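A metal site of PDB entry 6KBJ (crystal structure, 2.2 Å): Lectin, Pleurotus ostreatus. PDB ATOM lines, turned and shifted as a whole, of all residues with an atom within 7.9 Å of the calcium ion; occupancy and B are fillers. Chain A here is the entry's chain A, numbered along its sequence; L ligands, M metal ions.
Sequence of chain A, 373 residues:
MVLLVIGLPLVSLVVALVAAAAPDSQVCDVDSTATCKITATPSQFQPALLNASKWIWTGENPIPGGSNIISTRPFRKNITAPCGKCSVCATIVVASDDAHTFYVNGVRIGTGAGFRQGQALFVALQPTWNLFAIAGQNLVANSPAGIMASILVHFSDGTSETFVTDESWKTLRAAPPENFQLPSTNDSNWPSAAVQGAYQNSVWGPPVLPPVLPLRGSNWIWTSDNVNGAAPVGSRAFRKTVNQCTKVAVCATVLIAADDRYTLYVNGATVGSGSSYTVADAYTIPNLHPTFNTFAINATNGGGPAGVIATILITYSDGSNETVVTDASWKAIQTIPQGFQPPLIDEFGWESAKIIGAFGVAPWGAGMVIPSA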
ATOM      1  N   TRP A  57      -3.152  24.355  26.682  1.00  0.00           N
ATOM      2  CA  TRP A  57      -3.983  24.592  25.494  1.00  0.00           C
ATOM      3  C   TRP A  57      -3.021  24.739  24.333  1.00  0.00           C
ATOM      4  O   TRP A  57      -1.887  24.264  24.423  1.00  0.00           O
ATOM      5  CB  TRP A  57      -4.860  25.843  25.653  1.00  0.00           C
ATOM      6  CG  TRP A  57      -6.030  25.809  24.772  1.00  0.00           C
ATOM      7  CD1 TRP A  57      -6.340  26.703  23.768  1.00  0.00           C
ATOM      8  CD2 TRP A  57      -7.073  24.835  24.754  1.00  0.00           C
ATOM      9  NE1 TRP A  57      -7.488  26.369  23.177  1.00  0.00           N
ATOM     10  CE2 TRP A  57      -7.963  25.209  23.737  1.00  0.00           C
ATOM     11  CE3 TRP A  57      -7.324  23.688  25.492  1.00  0.00           C
ATOM     12  CZ2 TRP A  57      -9.101  24.475  23.437  1.00  0.00           C
ATOM     13  CZ3 TRP A  57      -8.458  22.948  25.198  1.00  0.00           C
ATOM     14  CH2 TRP A  57      -9.339  23.365  24.189  1.00  0.00           C
ATOM     15  N   GLY A  66      -5.946  33.550  28.328  1.00  0.00           N
ATOM     16  CA  GLY A  66      -6.563  34.537  27.517  1.00  0.00           C
ATOM     17  C   GLY A  66      -7.842  33.968  26.830  1.00  0.00           C
ATOM     18  O   GLY A  66      -8.127  32.726  26.901  1.00  0.00           O
ATOM     19  N   ASN A  68     -10.149  32.480  24.019  1.00  0.00           N
ATOM     20  CA  ASN A  68     -10.039  31.520  22.969  1.00  0.00           C
ATOM     21  C   ASN A  68     -11.427  31.305  22.287  1.00  0.00           C
ATOM     22  O   ASN A  68     -12.496  31.576  22.875  1.00  0.00           O
ATOM     23  CB  ASN A  68      -9.489  30.180  23.498  1.00  0.00           C
ATOM     24  CG  ASN A  68      -7.988  30.291  23.839  1.00  0.00           C
ATOM     25  OD1 ASN A  68      -7.602  30.741  24.954  1.00  0.00           O
ATOM     26  ND2 ASN A  68      -7.211  29.850  22.988  1.00  0.00           N
ATOM     27  N   ILE A  69     -11.349  30.797  21.079  1.00  0.00           N
ATOM     28  CA  ILE A  69     -12.546  30.497  20.282  1.00  0.00           C
ATOM     29  C   ILE A  69     -13.135  29.146  20.706  1.00  0.00           C
ATOM     30  O   ILE A  69     -12.423  28.300  21.238  1.00  0.00           O
ATOM     31  CB  ILE A  69     -12.208  30.512  18.765  1.00  0.00           C
ATOM     32  CG1 ILE A  69     -11.276  29.353  18.390  1.00  0.00           C
ATOM     33  CG2 ILE A  69     -11.579  31.892  18.305  1.00  0.00           C
ATOM     34  CD1 ILE A  69     -11.196  29.070  16.867  1.00  0.00           C
ATOM     35  N   ILE A  70     -14.398  28.934  20.372  1.00  0.00           N
ATOM     36  CA  ILE A  70     -15.067  27.660  20.588  1.00  0.00           C
ATOM     37  C   ILE A  70     -14.358  26.671  19.726  1.00  0.00           C
ATOM     38  O   ILE A  70     -14.197  26.909  18.576  1.00  0.00           O
ATOM     39  CB  ILE A  70     -16.561  27.747  20.182  1.00  0.00           C
ATOM     40  CG1 ILE A  70     -17.274  28.576  21.246  1.00  0.00           C
ATOM     41  CG2 ILE A  70     -17.207  26.375  20.062  1.00  0.00           C
ATOM     42  CD1 ILE A  70     -18.644  29.017  20.862  1.00  0.00           C
ATOM     43  N   SER A  96     -10.886  20.446  33.439  1.00  0.00           N
ATOM     44  CA  SER A  96     -10.900  21.134  32.126  1.00  0.00           C
ATOM     45  C   SER A  96     -11.789  22.381  32.126  1.00  0.00           C
ATOM     46  O   SER A  96     -12.772  22.503  32.809  1.00  0.00           O
ATOM     47  CB  SER A  96     -11.386  20.225  30.950  1.00  0.00           C
ATOM     48  OG  SER A  96     -12.743  19.745  31.314  1.00  0.00           O
ATOM     49  N   ASP A  97     -11.398  23.281  31.278  1.00  0.00           N
ATOM     50  CA  ASP A  97     -12.169  24.402  30.870  1.00  0.00           C
ATOM     51  C   ASP A  97     -12.292  24.275  29.331  1.00  0.00           C
ATOM     52  O   ASP A  97     -11.327  24.652  28.643  1.00  0.00           O
ATOM     53  CB  ASP A  97     -11.484  25.700  31.207  1.00  0.00           C
ATOM     54  CG  ASP A  97     -12.360  26.895  30.905  1.00  0.00           C
ATOM     55  OD1 ASP A  97     -13.339  26.787  30.124  1.00  0.00           O
ATOM     56  OD2 ASP A  97     -12.091  27.963  31.450  1.00  0.00           O
ATOM     57  N   ASP A  98     -13.452  23.797  28.787  1.00  0.00           N
ATOM     58  CA  ASP A  98     -14.671  23.445  29.536  1.00  0.00           C
ATOM     59  C   ASP A  98     -14.945  21.956  29.691  1.00  0.00           C
ATOM     60  O   ASP A  98     -15.661  21.561  30.604  1.00  0.00           O
ATOM     61  CB  ASP A  98     -15.918  24.064  28.836  1.00  0.00           C
ATOM     62  CG  ASP A  98     -15.874  25.576  28.743  1.00  0.00           C
ATOM     63  OD1 ASP A  98     -16.368  26.268  29.629  1.00  0.00           O
ATOM     64  OD2 ASP A  98     -15.448  26.126  27.666  1.00  0.00           O
ATOM     65  N   ALA A  99     -14.389  21.119  28.798  1.00  0.00           N
ATOM     66  CA  ALA A  99     -14.725  19.706  28.793  1.00  0.00           C
ATOM     67  C   ALA A  99     -13.634  18.867  28.232  1.00  0.00           C
ATOM     68  O   ALA A  99     -12.799  19.369  27.477  1.00  0.00           O
ATOM     69  CB  ALA A  99     -16.105  19.492  28.008  1.00  0.00           C
ATOM     70  N   PHE A 115     -13.536  23.059  35.880  1.00  0.00           N
ATOM     71  CA  PHE A 115     -12.196  23.380  36.422  1.00  0.00           C
ATOM     72  C   PHE A 115     -12.171  23.542  37.927  1.00  0.00           C
ATOM     73  O   PHE A 115     -11.139  23.537  38.505  1.00  0.00           O
ATOM     74  CB  PHE A 115     -11.651  24.591  35.715  1.00  0.00           C
ATOM     75  CG  PHE A 115     -12.499  25.849  35.880  1.00  0.00           C
ATOM     76  CD1 PHE A 115     -12.323  26.679  37.003  1.00  0.00           C
ATOM     77  CD2 PHE A 115     -13.396  26.238  34.868  1.00  0.00           C
ATOM     78  CE1 PHE A 115     -13.095  27.826  37.158  1.00  0.00           C
ATOM     79  CE2 PHE A 115     -14.187  27.419  35.006  1.00  0.00           C
ATOM     80  CZ  PHE A 115     -14.074  28.171  36.174  1.00  0.00           C
ATOM     81  N   GLN A 137     -12.260  20.704  24.928  1.00  0.00           N
ATOM     82  CA  GLN A 137     -13.148  21.596  24.249  1.00  0.00           C
ATOM     83  C   GLN A 137     -13.351  22.869  25.026  1.00  0.00           C
ATOM     84  O   GLN A 137     -13.699  22.847  26.193  1.00  0.00           O
ATOM     85  CB  GLN A 137     -14.577  21.016  24.060  1.00  0.00           C
ATOM     86  CG  GLN A 137     -14.665  19.641  23.404  1.00  0.00           C
ATOM     87  CD  GLN A 137     -16.144  19.107  23.514  1.00  0.00           C
ATOM     88  OE1 GLN A 137     -16.387  18.037  24.074  1.00  0.00           O
ATOM     89  NE2 GLN A 137     -17.114  19.940  23.082  1.00  0.00           N
ATOM     90  N   ASN A 138     -13.202  23.951  24.306  1.00  0.00           N
ATOM     91  CA  ASN A 138     -13.693  25.199  24.737  1.00  0.00           C
ATOM     92  C   ASN A 138     -15.123  25.422  24.179  1.00  0.00           C
ATOM     93  O   ASN A 138     -15.343  25.429  22.943  1.00  0.00           O
ATOM     94  CB  ASN A 138     -12.793  26.312  24.214  1.00  0.00           C
ATOM     95  CG  ASN A 138     -13.079  27.608  24.865  1.00  0.00           C
ATOM     96  OD1 ASN A 138     -13.562  27.600  25.980  1.00  0.00           O
ATOM     97  ND2 ASN A 138     -12.726  28.728  24.225  1.00  0.00           N
ATOM     98  N   LEU A 139     -16.044  25.682  25.077  1.00  0.00           N
ATOM     99  CA  LEU A 139     -17.486  25.745  24.724  1.00  0.00           C
ATOM    100  C   LEU A 139     -18.026  27.150  24.788  1.00  0.00           C
ATOM    101  O   LEU A 139     -19.105  27.316  24.338  1.00  0.00           O
ATOM    102  CB  LEU A 139     -18.343  24.877  25.686  1.00  0.00           C
ATOM    103  CG  LEU A 139     -18.090  23.350  25.634  1.00  0.00           C
ATOM    104  CD1 LEU A 139     -18.916  22.587  26.708  1.00  0.00           C
ATOM    105  CD2 LEU A 139     -18.253  22.770  24.230  1.00  0.00           C
ATOM    106  N   VAL A 140     -17.298  28.123  25.338  1.00  0.00           N
ATOM    107  CA  VAL A 140     -17.808  29.485  25.404  1.00  0.00           C
ATOM    108  C   VAL A 140     -16.874  30.402  24.639  1.00  0.00           C
ATOM    109  O   VAL A 140     -15.635  30.376  24.821  1.00  0.00           O
ATOM    110  CB  VAL A 140     -17.936  29.903  26.859  1.00  0.00           C
ATOM    111  CG1 VAL A 140     -18.420  31.306  26.980  1.00  0.00           C
ATOM    112  CG2 VAL A 140     -18.898  28.965  27.560  1.00  0.00           C
ATOM    113  N   ALA A 141     -17.457  31.251  23.813  1.00  0.00           N
ATOM    114  CA  ALA A 141     -16.654  32.159  22.988  1.00  0.00           C
ATOM    115  C   ALA A 141     -15.954  33.197  23.831  1.00  0.00           C
ATOM    116  O   ALA A 141     -16.501  33.655  24.830  1.00  0.00           O
ATOM    117  CB  ALA A 141     -17.516  32.841  21.941  1.00  0.00           C
ATOM    118  N   ASN A 142     -14.731  33.553  23.403  1.00  0.00           N
ATOM    119  CA  ASN A 142     -13.910  34.560  24.083  1.00  0.00           C
ATOM    120  C   ASN A 142     -13.547  34.177  25.552  1.00  0.00           C
ATOM    121  O   ASN A 142     -13.310  35.062  26.392  1.00  0.00           O
ATOM    122  CB  ASN A 142     -14.621  35.924  24.164  1.00  0.00           C
ATOM    123  CG  ASN A 142     -15.093  36.450  22.838  1.00  0.00           C
ATOM    124  OD1 ASN A 142     -14.353  36.546  21.882  1.00  0.00           O
ATOM    125  ND2 ASN A 142     -16.377  36.785  22.778  1.00  0.00           N
ATOM    126  N   SER A 143     -13.519  32.904  25.877  1.00  0.00           N
ATOM    127  CA  SER A 143     -13.308  32.536  27.246  1.00  0.00           C
ATOM    128  C   SER A 143     -11.976  31.765  27.312  1.00  0.00           C
ATOM    129  O   SER A 143     -11.484  31.275  26.324  1.00  0.00           O
ATOM    130  CB  SER A 143     -14.490  31.636  27.728  1.00  0.00           C
ATOM    131  OG  SER A 143     -14.437  30.402  27.046  1.00  0.00           O
ATOM    132  N   PRO A 144     -11.422  31.598  28.511  1.00  0.00           N
ATOM    133  CA  PRO A 144     -10.194  30.828  28.557  1.00  0.00           C
ATOM    134  C   PRO A 144     -10.401  29.370  28.288  1.00  0.00           C
ATOM    135  O   PRO A 144     -11.468  28.936  28.305  1.00  0.00           O
ATOM    136  CB  PRO A 144      -9.669  31.043  29.951  1.00  0.00           C
ATOM    137  CG  PRO A 144     -10.671  31.757  30.687  1.00  0.00           C
ATOM    138  CD  PRO A 144     -11.745  32.250  29.771  1.00  0.00           C
ATOM    139  N   ALA A 145      -9.336  28.667  27.952  1.00  0.00           N
ATOM    140  CA  ALA A 145      -9.399  27.271  27.656  1.00  0.00           C
ATOM    141  C   ALA A 145      -8.202  26.552  28.213  1.00  0.00           C
ATOM    142  O   ALA A 145      -7.056  27.077  28.213  1.00  0.00           O
ATOM    143  CB  ALA A 145      -9.446  27.076  26.160  1.00  0.00           C
ATOM    144  N   GLY A 146      -8.431  25.323  28.648  1.00  0.00           N
ATOM    145  CA  GLY A 146      -7.335  24.583  29.235  1.00  0.00           C
ATOM    146  C   GLY A 146      -7.703  23.265  29.829  1.00  0.00           C
ATOM    147  O   GLY A 146      -8.847  23.061  30.301  1.00  0.00           O
ATOM    148  N   TRP A 204      -7.815  30.025  36.778  1.00  0.00           N
ATOM    149  CA  TRP A 204      -8.760  29.056  37.356  1.00  0.00           C
ATOM    150  C   TRP A 204      -8.650  28.907  38.847  1.00  0.00           C
ATOM    151  O   TRP A 204      -9.602  28.595  39.487  1.00  0.00           O
ATOM    152  CB  TRP A 204      -8.610  27.715  36.642  1.00  0.00           C
ATOM    153  CG  TRP A 204      -8.924  27.855  35.184  1.00  0.00           C
ATOM    154  CD1 TRP A 204     -10.178  28.064  34.629  1.00  0.00           C
ATOM    155  CD2 TRP A 204      -8.015  27.860  34.118  1.00  0.00           C
ATOM    156  NE1 TRP A 204     -10.055  28.196  33.297  1.00  0.00           N
ATOM    157  CE2 TRP A 204      -8.738  28.044  32.945  1.00  0.00           C
ATOM    158  CE3 TRP A 204      -6.626  27.797  34.047  1.00  0.00           C
ATOM    159  CZ2 TRP A 204      -8.162  28.118  31.759  1.00  0.00           C
ATOM    160  CZ3 TRP A 204      -6.046  27.851  32.811  1.00  0.00           C
ATOM    161  CH2 TRP A 204      -6.799  27.984  31.677  1.00  0.00           C
HETATM  162  C1  LIG L   1     -14.668  30.279  32.185  1.00  0.00           C
HETATM  163  C2  LIG L   1     -15.922  30.578  33.006  1.00  0.00           C
HETATM  164  C3  LIG L   1     -14.911  29.550  30.753  1.00  0.00           C
HETATM  165  O1  LIG L   1     -15.849  30.908  34.265  1.00  0.00           O
HETATM  166  O2  LIG L   1     -16.969  30.400  32.322  1.00  0.00           O
HETATM  167  O3  LIG L   1     -16.005  29.010  30.017  1.00  0.00           O
HETATM  168  O4  LIG L   1     -13.759  29.632  30.337  1.00  0.00           O
HETATM  169 CA    CA M   1     -13.812  28.179  28.182  1.00  0.00          CA
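ND2 of Asn 138 lies within hydrogen-bond range of O of Val 140 (3.4 Å). The backbone carbonyl oxygen of Asn 68 sits at hydrogen-bond distance from the side-chain amide nitrogen of Asn 138. The side-chain amide nitrogen of Asn 138 lies within hydrogen-bond range of the backbone carbonyl oxygen of Ile 69 (3.0 Å). The backbone NH (N) of Asp 97 lies within hydrogen-bond range of the backbone carbonyl oxygen (O) of Gly 146, 2.7 Å away. NE1 of Trp 204 is in hydrogen-bond range of OD2 of Asp 97. The side-chain hydroxyl (OG) of Ser 143 sits close to the backbone carbonyl oxygen (O) of Val 140 (2.5 Å). O of Ser 143 sits at hydrogen-bond distance from N of Asn 68 (2.9 Å). OD2 of Asp 98 sits close to N of Leu 139, at 2.7 Å.
The calcium ion is bound by OD1 of Asn 138 (2.3 Å). The calcium ion is bound by the side-chain carboxylate (OD1) of Asp 97 (2.4 Å). The backbone carbonyl oxygen (O) of Pro 144 binds the calcium ion, 2.5 Å away. OG of Ser 143 is bound to the calcium ion, 2.6 Å away. O4 of the ligand is bound to the calcium ion, 2.6 Å away. The calcium ion is bound by OD2 of Asp 98 (2.7 Å). Slightly farther from the calcium ion lies an oxygen (O3) of the ligand (3.0 Å).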
